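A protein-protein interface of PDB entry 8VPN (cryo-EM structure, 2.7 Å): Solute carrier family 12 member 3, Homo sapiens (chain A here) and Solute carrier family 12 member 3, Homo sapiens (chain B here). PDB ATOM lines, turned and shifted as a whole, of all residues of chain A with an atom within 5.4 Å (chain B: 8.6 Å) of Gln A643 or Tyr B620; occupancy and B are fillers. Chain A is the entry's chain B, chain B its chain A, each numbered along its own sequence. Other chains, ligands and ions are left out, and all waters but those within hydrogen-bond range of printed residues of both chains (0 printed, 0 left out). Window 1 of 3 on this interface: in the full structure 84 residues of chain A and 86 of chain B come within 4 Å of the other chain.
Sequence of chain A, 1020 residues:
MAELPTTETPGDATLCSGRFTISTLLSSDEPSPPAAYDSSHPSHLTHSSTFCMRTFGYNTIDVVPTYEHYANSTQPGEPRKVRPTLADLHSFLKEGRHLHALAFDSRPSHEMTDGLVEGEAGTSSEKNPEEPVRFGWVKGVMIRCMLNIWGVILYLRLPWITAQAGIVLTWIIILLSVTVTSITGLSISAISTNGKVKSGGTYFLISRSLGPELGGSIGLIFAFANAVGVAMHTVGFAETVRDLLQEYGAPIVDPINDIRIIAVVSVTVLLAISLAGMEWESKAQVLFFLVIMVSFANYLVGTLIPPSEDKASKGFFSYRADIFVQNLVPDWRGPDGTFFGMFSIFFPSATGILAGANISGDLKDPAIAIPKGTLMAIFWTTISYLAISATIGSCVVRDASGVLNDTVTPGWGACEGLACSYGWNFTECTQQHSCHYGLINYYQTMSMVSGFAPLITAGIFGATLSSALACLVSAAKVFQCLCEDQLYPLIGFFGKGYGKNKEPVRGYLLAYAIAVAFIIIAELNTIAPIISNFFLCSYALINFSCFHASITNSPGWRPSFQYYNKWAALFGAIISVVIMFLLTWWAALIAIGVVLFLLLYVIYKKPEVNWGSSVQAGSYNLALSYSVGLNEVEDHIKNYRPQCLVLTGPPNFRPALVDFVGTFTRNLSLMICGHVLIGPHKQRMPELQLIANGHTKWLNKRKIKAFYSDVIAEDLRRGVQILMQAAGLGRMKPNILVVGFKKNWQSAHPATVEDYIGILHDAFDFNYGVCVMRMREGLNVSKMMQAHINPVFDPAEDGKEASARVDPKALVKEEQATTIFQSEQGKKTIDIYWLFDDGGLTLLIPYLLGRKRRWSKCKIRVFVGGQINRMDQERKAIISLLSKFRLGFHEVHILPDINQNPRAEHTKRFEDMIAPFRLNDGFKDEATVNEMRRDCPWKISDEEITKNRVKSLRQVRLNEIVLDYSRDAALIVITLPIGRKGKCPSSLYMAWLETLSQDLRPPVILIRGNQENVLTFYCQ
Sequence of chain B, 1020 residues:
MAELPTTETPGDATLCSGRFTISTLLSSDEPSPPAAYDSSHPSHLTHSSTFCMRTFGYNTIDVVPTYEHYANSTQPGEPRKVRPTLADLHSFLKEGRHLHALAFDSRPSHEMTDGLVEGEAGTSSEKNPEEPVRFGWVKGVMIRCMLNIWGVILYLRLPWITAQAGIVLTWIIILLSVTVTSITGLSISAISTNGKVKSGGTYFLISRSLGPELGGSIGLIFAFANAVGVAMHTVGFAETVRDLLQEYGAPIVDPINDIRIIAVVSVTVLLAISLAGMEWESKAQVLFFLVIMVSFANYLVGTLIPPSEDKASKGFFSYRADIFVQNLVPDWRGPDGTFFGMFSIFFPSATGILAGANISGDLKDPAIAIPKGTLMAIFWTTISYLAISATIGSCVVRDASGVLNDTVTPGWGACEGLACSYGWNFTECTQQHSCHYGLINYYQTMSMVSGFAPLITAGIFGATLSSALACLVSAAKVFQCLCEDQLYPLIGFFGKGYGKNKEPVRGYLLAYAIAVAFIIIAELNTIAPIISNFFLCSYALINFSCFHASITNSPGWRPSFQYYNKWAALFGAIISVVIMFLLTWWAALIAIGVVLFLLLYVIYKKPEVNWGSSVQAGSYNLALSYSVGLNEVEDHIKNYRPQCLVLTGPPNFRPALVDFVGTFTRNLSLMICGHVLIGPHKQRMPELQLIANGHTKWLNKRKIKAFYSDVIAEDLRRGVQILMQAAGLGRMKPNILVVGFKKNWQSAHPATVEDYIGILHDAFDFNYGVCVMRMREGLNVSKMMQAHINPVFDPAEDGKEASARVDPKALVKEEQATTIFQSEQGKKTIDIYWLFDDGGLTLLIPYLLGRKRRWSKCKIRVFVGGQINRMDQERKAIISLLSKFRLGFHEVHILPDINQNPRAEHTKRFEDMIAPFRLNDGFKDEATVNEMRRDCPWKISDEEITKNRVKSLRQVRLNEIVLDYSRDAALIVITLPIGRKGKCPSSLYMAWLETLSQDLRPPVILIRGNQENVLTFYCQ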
ATOM      1  N   LEU A 630      17.158 -13.988  17.797  1.00  0.00           N
ATOM      2  CA  LEU A 630      17.735 -13.195  18.882  1.00  0.00           C
ATOM      3  C   LEU A 630      19.257 -13.206  18.900  1.00  0.00           C
ATOM      4  O   LEU A 630      19.851 -12.451  19.675  1.00  0.00           O
ATOM      5  CB  LEU A 630      17.221 -13.687  20.237  1.00  0.00           C
ATOM      6  CG  LEU A 630      17.688 -12.883  21.452  1.00  0.00           C
ATOM      7  CD1 LEU A 630      17.087 -11.486  21.456  1.00  0.00           C
ATOM      8  CD2 LEU A 630      17.361 -13.625  22.737  1.00  0.00           C
ATOM      9  N   ARG A 641      18.254  -7.255  31.753  1.00  0.00           N
ATOM     10  CA  ARG A 641      17.169  -8.053  32.314  1.00  0.00           C
ATOM     11  C   ARG A 641      17.708  -9.064  33.317  1.00  0.00           C
ATOM     12  O   ARG A 641      18.737  -9.707  33.060  1.00  0.00           O
ATOM     13  CB  ARG A 641      16.394  -8.788  31.212  1.00  0.00           C
ATOM     14  CG  ARG A 641      15.220  -7.994  30.664  1.00  0.00           C
ATOM     15  CD  ARG A 641      14.694  -8.601  29.379  1.00  0.00           C
ATOM     16  NE  ARG A 641      13.253  -8.423  29.246  1.00  0.00           N
ATOM     17  CZ  ARG A 641      12.668  -7.597  28.391  1.00  0.00           C
ATOM     18  NH1 ARG A 641      13.370  -6.867  27.543  1.00  0.00           N
ATOM     19  NH2 ARG A 641      11.342  -7.512  28.378  1.00  0.00           N
ATOM     20  N   PRO A 642      17.046  -9.219  34.472  1.00  0.00           N
ATOM     21  CA  PRO A 642      17.472 -10.215  35.465  1.00  0.00           C
ATOM     22  C   PRO A 642      16.947 -11.606  35.143  1.00  0.00           C
ATOM     23  O   PRO A 642      15.754 -11.886  35.295  1.00  0.00           O
ATOM     24  CB  PRO A 642      16.879  -9.671  36.773  1.00  0.00           C
ATOM     25  CG  PRO A 642      15.690  -8.895  36.355  1.00  0.00           C
ATOM     26  CD  PRO A 642      15.917  -8.402  34.951  1.00  0.00           C
ATOM     27  N   GLN A 643      17.849 -12.493  34.725  1.00  0.00           N
ATOM     28  CA  GLN A 643      17.537 -13.901  34.510  1.00  0.00           C
ATOM     29  C   GLN A 643      17.839 -14.656  35.798  1.00  0.00           C
ATOM     30  O   GLN A 643      18.975 -14.627  36.281  1.00  0.00           O
ATOM     31  CB  GLN A 643      18.353 -14.479  33.356  1.00  0.00           C
ATOM     32  CG  GLN A 643      17.700 -14.381  31.993  1.00  0.00           C
ATOM     33  CD  GLN A 643      18.134 -13.151  31.237  1.00  0.00           C
ATOM     34  OE1 GLN A 643      18.441 -12.127  31.834  1.00  0.00           O
ATOM     35  NE2 GLN A 643      18.168 -13.247  29.917  1.00  0.00           N
ATOM     36  N   CYS A 644      16.837 -15.341  36.337  1.00  0.00           N
ATOM     37  CA  CYS A 644      16.912 -15.915  37.672  1.00  0.00           C
ATOM     38  C   CYS A 644      16.941 -17.436  37.621  1.00  0.00           C
ATOM     39  O   CYS A 644      16.133 -18.058  36.920  1.00  0.00           O
ATOM     40  CB  CYS A 644      15.734 -15.445  38.528  1.00  0.00           C
ATOM     41  SG  CYS A 644      15.925 -13.781  39.197  1.00  0.00           S
ATOM     42  N   LEU A 645      17.877 -18.019  38.369  1.00  0.00           N
ATOM     43  CA  LEU A 645      17.940 -19.450  38.640  1.00  0.00           C
ATOM     44  C   LEU A 645      17.605 -19.654  40.115  1.00  0.00           C
ATOM     45  O   LEU A 645      18.360 -19.220  40.991  1.00  0.00           O
ATOM     46  CB  LEU A 645      19.325 -19.994  38.297  1.00  0.00           C
ATOM     47  CG  LEU A 645      19.695 -21.396  38.776  1.00  0.00           C
ATOM     48  CD1 LEU A 645      18.967 -22.444  37.962  1.00  0.00           C
ATOM     49  CD2 LEU A 645      21.198 -21.608  38.716  1.00  0.00           C
ATOM     50  N   LEU A 668       8.540 -10.586  31.914  1.00  0.00           N
ATOM     51  CA  LEU A 668       9.610  -9.610  31.754  1.00  0.00           C
ATOM     52  C   LEU A 668      10.968 -10.247  31.499  1.00  0.00           C
ATOM     53  O   LEU A 668      11.759  -9.690  30.734  1.00  0.00           O
ATOM     54  CB  LEU A 668       9.694  -8.686  32.977  1.00  0.00           C
ATOM     55  CG  LEU A 668      10.738  -7.573  32.835  1.00  0.00           C
ATOM     56  CD1 LEU A 668      10.129  -6.199  33.038  1.00  0.00           C
ATOM     57  CD2 LEU A 668      11.885  -7.802  33.798  1.00  0.00           C
ATOM     58  N   SER A 669      11.264 -11.386  32.121  1.00  0.00           N
ATOM     59  CA  SER A 669      12.559 -12.036  31.941  1.00  0.00           C
ATOM     60  C   SER A 669      12.411 -13.525  32.238  1.00  0.00           C
ATOM     61  O   SER A 669      11.304 -14.028  32.457  1.00  0.00           O
ATOM     62  CB  SER A 669      13.630 -11.380  32.818  1.00  0.00           C
ATOM     63  OG  SER A 669      13.458 -11.720  34.183  1.00  0.00           O
ATOM     64  N   LEU A 670      13.541 -14.226  32.263  1.00  0.00           N
ATOM     65  CA  LEU A 670      13.597 -15.679  32.324  1.00  0.00           C
ATOM     66  C   LEU A 670      13.645 -16.177  33.765  1.00  0.00           C
ATOM     67  O   LEU A 670      14.234 -15.541  34.642  1.00  0.00           O
ATOM     68  CB  LEU A 670      14.823 -16.175  31.558  1.00  0.00           C
ATOM     69  CG  LEU A 670      15.232 -17.641  31.660  1.00  0.00           C
ATOM     70  CD1 LEU A 670      14.309 -18.512  30.834  1.00  0.00           C
ATOM     71  CD2 LEU A 670      16.662 -17.796  31.210  1.00  0.00           C
ATOM     72  N   ARG A 731      21.581 -16.245  24.151  1.00  0.00           N
ATOM     73  CA  ARG A 731      21.589 -15.083  25.030  1.00  0.00           C
ATOM     74  C   ARG A 731      20.563 -15.176  26.147  1.00  0.00           C
ATOM     75  O   ARG A 731      20.486 -14.264  26.975  1.00  0.00           O
ATOM     76  CB  ARG A 731      21.349 -13.805  24.219  1.00  0.00           C
ATOM     77  CG  ARG A 731      22.417 -13.560  23.175  1.00  0.00           C
ATOM     78  CD  ARG A 731      22.416 -12.142  22.657  1.00  0.00           C
ATOM     79  NE  ARG A 731      23.386 -11.984  21.581  1.00  0.00           N
ATOM     80  CZ  ARG A 731      24.500 -11.273  21.681  1.00  0.00           C
ATOM     81  NH1 ARG A 731      24.809 -10.624  22.791  1.00  0.00           N
ATOM     82  NH2 ARG A 731      25.326 -11.212  20.640  1.00  0.00           N
ATOM     83  N   MET A 732      19.773 -16.241  26.188  1.00  0.00           N
ATOM     84  CA  MET A 732      18.798 -16.438  27.253  1.00  0.00           C
ATOM     85  C   MET A 732      19.399 -17.339  28.331  1.00  0.00           C
ATOM     86  O   MET A 732      19.015 -18.491  28.509  1.00  0.00           O
ATOM     87  CB  MET A 732      17.509 -17.021  26.683  1.00  0.00           C
ATOM     88  CG  MET A 732      16.260 -16.195  26.966  1.00  0.00           C
ATOM     89  SD  MET A 732      14.799 -16.889  26.178  1.00  0.00           S
ATOM     90  CE  MET A 732      15.046 -16.356  24.490  1.00  0.00           C
ATOM     91  N   LYS A 733      20.366 -16.785  29.054  1.00  0.00           N
ATOM     92  CA  LYS A 733      21.031 -17.535  30.108  1.00  0.00           C
ATOM     93  C   LYS A 733      21.044 -16.741  31.405  1.00  0.00           C
ATOM     94  O   LYS A 733      21.220 -15.520  31.393  1.00  0.00           O
ATOM     95  CB  LYS A 733      22.468 -17.901  29.705  1.00  0.00           C
ATOM     96  CG  LYS A 733      23.489 -16.804  29.910  1.00  0.00           C
ATOM     97  CD  LYS A 733      24.508 -16.794  28.787  1.00  0.00           C
ATOM     98  CE  LYS A 733      25.771 -16.070  29.207  1.00  0.00           C
ATOM     99  NZ  LYS A 733      26.880 -17.036  29.457  1.00  0.00           N
ATOM    100  N   PRO A 734      20.892 -17.418  32.541  1.00  0.00           N
ATOM    101  CA  PRO A 734      20.726 -16.712  33.816  1.00  0.00           C
ATOM    102  C   PRO A 734      21.990 -15.990  34.257  1.00  0.00           C
ATOM    103  O   PRO A 734      23.107 -16.324  33.862  1.00  0.00           O
ATOM    104  CB  PRO A 734      20.367 -17.831  34.797  1.00  0.00           C
ATOM    105  CG  PRO A 734      20.937 -19.057  34.192  1.00  0.00           C
ATOM    106  CD  PRO A 734      20.843 -18.881  32.707  1.00  0.00           C
ATOM    107  N   ASN A 735      21.785 -14.973  35.100  1.00  0.00           N
ATOM    108  CA  ASN A 735      22.894 -14.260  35.721  1.00  0.00           C
ATOM    109  C   ASN A 735      22.641 -13.948  37.194  1.00  0.00           C
ATOM    110  O   ASN A 735      23.415 -13.188  37.789  1.00  0.00           O
ATOM    111  CB  ASN A 735      23.200 -12.965  34.955  1.00  0.00           C
ATOM    112  CG  ASN A 735      21.960 -12.143  34.673  1.00  0.00           C
ATOM    113  OD1 ASN A 735      20.982 -12.204  35.412  1.00  0.00           O
ATOM    114  ND2 ASN A 735      21.993 -11.372  33.594  1.00  0.00           N
ATOM    115  N   ILE A 736      21.598 -14.511  37.801  1.00  0.00           N
ATOM    116  CA  ILE A 736      21.289 -14.311  39.212  1.00  0.00           C
ATOM    117  C   ILE A 736      20.883 -15.646  39.820  1.00  0.00           C
ATOM    118  O   ILE A 736      20.200 -16.450  39.177  1.00  0.00           O
ATOM    119  CB  ILE A 736      20.177 -13.261  39.412  1.00  0.00           C
ATOM    120  CG1 ILE A 736      20.488 -11.997  38.612  1.00  0.00           C
ATOM    121  CG2 ILE A 736      19.994 -12.939  40.885  1.00  0.00           C
ATOM    122  CD1 ILE A 736      19.446 -10.924  38.737  1.00  0.00           C
ATOM    123  N   THR B 552       6.185  -1.833  24.539  1.00  0.00           N
ATOM    124  CA  THR B 552       7.209  -2.836  24.824  1.00  0.00           C
ATOM    125  C   THR B 552       7.470  -2.950  26.323  1.00  0.00           C
ATOM    126  O   THR B 552       7.484  -4.052  26.881  1.00  0.00           O
ATOM    127  CB  THR B 552       8.496  -2.505  24.072  1.00  0.00           C
ATOM    128  OG1 THR B 552       8.355  -2.890  22.701  1.00  0.00           O
ATOM    129  CG2 THR B 552       9.660  -3.263  24.675  1.00  0.00           C
ATOM    130  N   SER B 554      10.212  -2.104  28.469  1.00  0.00           N
ATOM    131  CA  SER B 554      11.444  -2.659  28.998  1.00  0.00           C
ATOM    132  C   SER B 554      11.770  -2.026  30.348  1.00  0.00           C
ATOM    133  O   SER B 554      11.284  -0.940  30.673  1.00  0.00           O
ATOM    134  CB  SER B 554      12.585  -2.447  28.011  1.00  0.00           C
ATOM    135  OG  SER B 554      13.327  -1.283  28.317  1.00  0.00           O
ATOM    136  N   PRO B 555      12.580  -2.697  31.170  1.00  0.00           N
ATOM    137  CA  PRO B 555      12.912  -2.130  32.488  1.00  0.00           C
ATOM    138  C   PRO B 555      13.709  -0.839  32.415  1.00  0.00           C
ATOM    139  O   PRO B 555      13.814  -0.141  33.429  1.00  0.00           O
ATOM    140  CB  PRO B 555      13.712  -3.253  33.161  1.00  0.00           C
ATOM    141  CG  PRO B 555      14.253  -4.057  32.042  1.00  0.00           C
ATOM    142  CD  PRO B 555      13.223  -4.004  30.954  1.00  0.00           C
ATOM    143  N   SER B 613      17.404   0.299  21.638  1.00  0.00           N
ATOM    144  CA  SER B 613      16.127   0.709  21.078  1.00  0.00           C
ATOM    145  C   SER B 613      15.034  -0.258  21.508  1.00  0.00           C
ATOM    146  O   SER B 613      15.295  -1.319  22.078  1.00  0.00           O
ATOM    147  CB  SER B 613      16.202   0.797  19.551  1.00  0.00           C
ATOM    148  OG  SER B 613      17.289   1.614  19.152  1.00  0.00           O
ATOM    149  N   SER B 614      13.790   0.134  21.234  1.00  0.00           N
ATOM    150  CA  SER B 614      12.661  -0.721  21.566  1.00  0.00           C
ATOM    151  C   SER B 614      12.590  -1.948  20.669  1.00  0.00           C
ATOM    152  O   SER B 614      11.941  -2.933  21.036  1.00  0.00           O
ATOM    153  CB  SER B 614      11.356   0.076  21.483  1.00  0.00           C
ATOM    154  OG  SER B 614      11.335   0.921  20.351  1.00  0.00           O
ATOM    155  N   VAL B 615      13.264  -1.924  19.516  1.00  0.00           N
ATOM    156  CA  VAL B 615      13.216  -3.060  18.601  1.00  0.00           C
ATOM    157  C   VAL B 615      13.966  -4.257  19.178  1.00  0.00           C
ATOM    158  O   VAL B 615      13.484  -5.396  19.117  1.00  0.00           O
ATOM    159  CB  VAL B 615      13.770  -2.654  17.222  1.00  0.00           C
ATOM    160  CG1 VAL B 615      13.303  -3.622  16.161  1.00  0.00           C
ATOM    161  CG2 VAL B 615      13.338  -1.242  16.872  1.00  0.00           C
ATOM    162  N   GLN B 616      15.158  -4.029  19.737  1.00  0.00           N
ATOM    163  CA  GLN B 616      15.930  -5.128  20.314  1.00  0.00           C
ATOM    164  C   GLN B 616      15.221  -5.722  21.526  1.00  0.00           C
ATOM    165  O   GLN B 616      15.182  -6.951  21.706  1.00  0.00           O
ATOM    166  CB  GLN B 616      17.327  -4.635  20.690  1.00  0.00           C
ATOM    167  CG  GLN B 616      17.629  -3.236  20.174  1.00  0.00           C
ATOM    168  CD  GLN B 616      19.114  -2.971  19.983  1.00  0.00           C
ATOM    169  OE1 GLN B 616      19.961  -3.672  20.534  1.00  0.00           O
ATOM    170  NE2 GLN B 616      19.432  -1.956  19.190  1.00  0.00           N
ATOM    171  N   ALA B 617      14.653  -4.858  22.367  1.00  0.00           N
ATOM    172  CA  ALA B 617      13.863  -5.338  23.491  1.00  0.00           C
ATOM    173  C   ALA B 617      12.667  -6.145  23.008  1.00  0.00           C
ATOM    174  O   ALA B 617      12.306  -7.156  23.618  1.00  0.00           O
ATOM    175  CB  ALA B 617      13.413  -4.162  24.354  1.00  0.00           C
ATOM    176  N   GLY B 618      12.037  -5.711  21.914  1.00  0.00           N
ATOM    177  CA  GLY B 618      10.945  -6.485  21.350  1.00  0.00           C
ATOM    178  C   GLY B 618      11.385  -7.850  20.859  1.00  0.00           C
ATOM    179  O   GLY B 618      10.653  -8.832  20.984  1.00  0.00           O
ATOM    180  N   SER B 619      12.577  -7.926  20.268  1.00  0.00           N
ATOM    181  CA  SER B 619      13.079  -9.223  19.822  1.00  0.00           C
ATOM    182  C   SER B 619      13.272 -10.168  21.004  1.00  0.00           C
ATOM    183  O   SER B 619      12.888 -11.345  20.941  1.00  0.00           O
ATOM    184  CB  SER B 619      14.382  -9.050  19.044  1.00  0.00           C
ATOM    185  OG  SER B 619      15.313  -8.273  19.767  1.00  0.00           O
ATOM    186  N   TYR B 620      13.848  -9.666  22.100  1.00  0.00           N
ATOM    187  CA  TYR B 620      13.938 -10.498  23.301  1.00  0.00           C
ATOM    188  C   TYR B 620      12.551 -10.896  23.797  1.00  0.00           C
ATOM    189  O   TYR B 620      12.332 -12.046  24.206  1.00  0.00           O
ATOM    190  CB  TYR B 620      14.711  -9.785  24.410  1.00  0.00           C
ATOM    191  CG  TYR B 620      14.887 -10.635  25.656  1.00  0.00           C
ATOM    192  CD1 TYR B 620      13.894 -10.706  26.619  1.00  0.00           C
ATOM    193  CD2 TYR B 620      16.037 -11.383  25.855  1.00  0.00           C
ATOM    194  CE1 TYR B 620      14.043 -11.483  27.745  1.00  0.00           C
ATOM    195  CE2 TYR B 620      16.197 -12.165  26.982  1.00  0.00           C
ATOM    196  CZ  TYR B 620      15.195 -12.209  27.924  1.00  0.00           C
ATOM    197  OH  TYR B 620      15.341 -12.985  29.047  1.00  0.00           O
ATOM    198  N   ASN B 621      11.610  -9.950  23.787  1.00  0.00           N
ATOM    199  CA  ASN B 621      10.242 -10.228  24.208  1.00  0.00           C
ATOM    200  C   ASN B 621       9.650 -11.392  23.426  1.00  0.00           C
ATOM    201  O   ASN B 621       9.071 -12.317  24.001  1.00  0.00           O
ATOM    202  CB  ASN B 621       9.385  -8.972  24.018  1.00  0.00           C
ATOM    203  CG  ASN B 621       9.301  -8.114  25.265  1.00  0.00           C
ATOM    204  OD1 ASN B 621      10.314  -7.646  25.788  1.00  0.00           O
ATOM    205  ND2 ASN B 621       8.085  -7.874  25.727  1.00  0.00           N
ATOM    206  N   LEU B 622       9.776 -11.346  22.098  1.00  0.00           N
ATOM    207  CA  LEU B 622       9.202 -12.390  21.253  1.00  0.00           C
ATOM    208  C   LEU B 622       9.876 -13.733  21.493  1.00  0.00           C
ATOM    209  O   LEU B 622       9.200 -14.769  21.573  1.00  0.00           O
ATOM    210  CB  LEU B 622       9.318 -11.993  19.785  1.00  0.00           C
ATOM    211  CG  LEU B 622       8.410 -10.852  19.341  1.00  0.00           C
ATOM    212  CD1 LEU B 622       9.136  -9.974  18.341  1.00  0.00           C
ATOM    213  CD2 LEU B 622       7.147 -11.407  18.733  1.00  0.00           C
ATOM    214  N   ALA B 623      11.207 -13.742  21.597  1.00  0.00           N
ATOM    215  CA  ALA B 623      11.901 -14.994  21.886  1.00  0.00           C
ATOM    216  C   ALA B 623      11.371 -15.626  23.170  1.00  0.00           C
ATOM    217  O   ALA B 623      11.012 -16.814  23.196  1.00  0.00           O
ATOM    218  CB  ALA B 623      13.405 -14.743  21.976  1.00  0.00           C
ATOM    219  N   LEU B 624      11.285 -14.834  24.241  1.00  0.00           N
ATOM    220  CA  LEU B 624      10.822 -15.367  25.519  1.00  0.00           C
ATOM    221  C   LEU B 624       9.375 -15.845  25.431  1.00  0.00           C
ATOM    222  O   LEU B 624       9.037 -16.929  25.926  1.00  0.00           O
ATOM    223  CB  LEU B 624      10.977 -14.302  26.606  1.00  0.00           C
ATOM    224  CG  LEU B 624      10.554 -14.619  28.040  1.00  0.00           C
ATOM    225  CD1 LEU B 624      11.142 -15.939  28.504  1.00  0.00           C
ATOM    226  CD2 LEU B 624      10.958 -13.488  28.969  1.00  0.00           C
ATOM    227  N   SER B 625       8.510 -15.050  24.797  1.00  0.00           N
ATOM    228  CA  SER B 625       7.092 -15.388  24.722  1.00  0.00           C
ATOM    229  C   SER B 625       6.866 -16.686  23.959  1.00  0.00           C
ATOM    230  O   SER B 625       6.068 -17.530  24.385  1.00  0.00           O
ATOM    231  CB  SER B 625       6.321 -14.240  24.074  1.00  0.00           C
ATOM    232  OG  SER B 625       4.986 -14.610  23.798  1.00  0.00           O
ATOM    233  N   TYR B 626       7.559 -16.872  22.835  1.00  0.00           N
ATOM    234  CA  TYR B 626       7.363 -18.098  22.068  1.00  0.00           C
ATOM    235  C   TYR B 626       7.984 -19.307  22.752  1.00  0.00           C
ATOM    236  O   TYR B 626       7.435 -20.412  22.659  1.00  0.00           O
ATOM    237  CB  TYR B 626       7.912 -17.936  20.655  1.00  0.00           C
ATOM    238  CG  TYR B 626       6.959 -17.184  19.763  1.00  0.00           C
ATOM    239  CD1 TYR B 626       5.697 -17.691  19.477  1.00  0.00           C
ATOM    240  CD2 TYR B 626       7.305 -15.956  19.233  1.00  0.00           C
ATOM    241  CE1 TYR B 626       4.818 -16.996  18.675  1.00  0.00           C
ATOM    242  CE2 TYR B 626       6.434 -15.257  18.434  1.00  0.00           C
ATOM    243  CZ  TYR B 626       5.197 -15.780  18.154  1.00  0.00           C
ATOM    244  OH  TYR B 626       4.335 -15.073  17.350  1.00  0.00           O
ATOM    245  N   SER B 627       9.114 -19.136  23.444  1.00  0.00           N
ATOM    246  CA  SER B 627       9.635 -20.247  24.234  1.00  0.00           C
ATOM    247  C   SER B 627       8.619 -20.690  25.281  1.00  0.00           C
ATOM    248  O   SER B 627       8.335 -21.887  25.428  1.00  0.00           O
ATOM    249  CB  SER B 627      10.953 -19.850  24.895  1.00  0.00           C
ATOM    250  OG  SER B 627      12.030 -19.950  23.985  1.00  0.00           O
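OH of Tyr B620 lies within hydrogen-bond range of NE2 of Gln A643, at 3.0 Å.
The side-chain amide oxygen (OD1) of Asn B621 is in hydrogen-bond range of the guanidinium group (NH2) of Arg A641, at 2.8 Å.
O of Ala B617 sits close to OD1 of Asn B621, 3.0 Å away.
O of Arg A641 lies close to OE1 of Gln A643 (2.7 Å).
NE of Arg A641 is in hydrogen-bond range of O of Leu A668, at 2.5 Å.
N of Asn A735 sits at hydrogen-bond distance from O of Gln A643.
The backbone carbonyl oxygen (O) of Gln A643 is in hydrogen-bond range of the backbone NH (N) of Ile A736.
The backbone carbonyl oxygen of Leu A670 lies within hydrogen-bond range of the backbone NH of Cys A644 (3.1 Å).
N of Tyr B620 touches CD1 of Leu A630, 3.8 Å away.
CD of Arg A641 touches CE1 of Tyr B620 (3.4 Å).
O of Ser A669 touches CD2 of Leu B624, at 3.5 Å.
N of Leu A670 touches OH of Tyr B620 (3.9 Å).
Met A732 touches Tyr B620.
Met A732 touches Ala B623.
Of chain B, only Tyr B620 (3.0 Å) comes within 4 Å of Gln A643.
Of chain A, only Leu A630, Arg A641, Gln A643, Leu A670 and Met A732 come within 4 Å of Tyr B620.
No residue of chain B comes within 4 Å of Pro A642.
Of the printed residues of chain A, Leu B624 touches Ser A669 (3.5 Å).
Printed residues of chain B within 4 Å of Met A732: Tyr B620 and Ala B623.
Of the printed residues of chain B, Ser A669 touches Leu B624.
Printed residues of chain B within 4 Å of Arg A641: Tyr B620 (3.4 Å) and Asn B621 (2.8 Å).
Pro A734 touches none of the printed residues of chain B.
The nearest printed residue of chain B that does not touch Leu A630 is Ser B619 (4.04 Å).
Printed residues of chain B that touch a printed residue of chain A: Tyr B620, Asn B621, Ala B623 and Leu B624.
Of the 15 printed residues of chain A, 6 touch a printed residue of chain B.
Hydrophobic or aromatic side chains of chain A within 4 Å of the printed part of chain B: Leu A630 and Met A732.
Along chain A the printed residues that touch a printed residue of chain B span positions 630 to 732.
Among the printed residues, no Asp or Glu carboxylate lies within 4 Å of a Lys or Arg side-chain nitrogen of the other chain.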
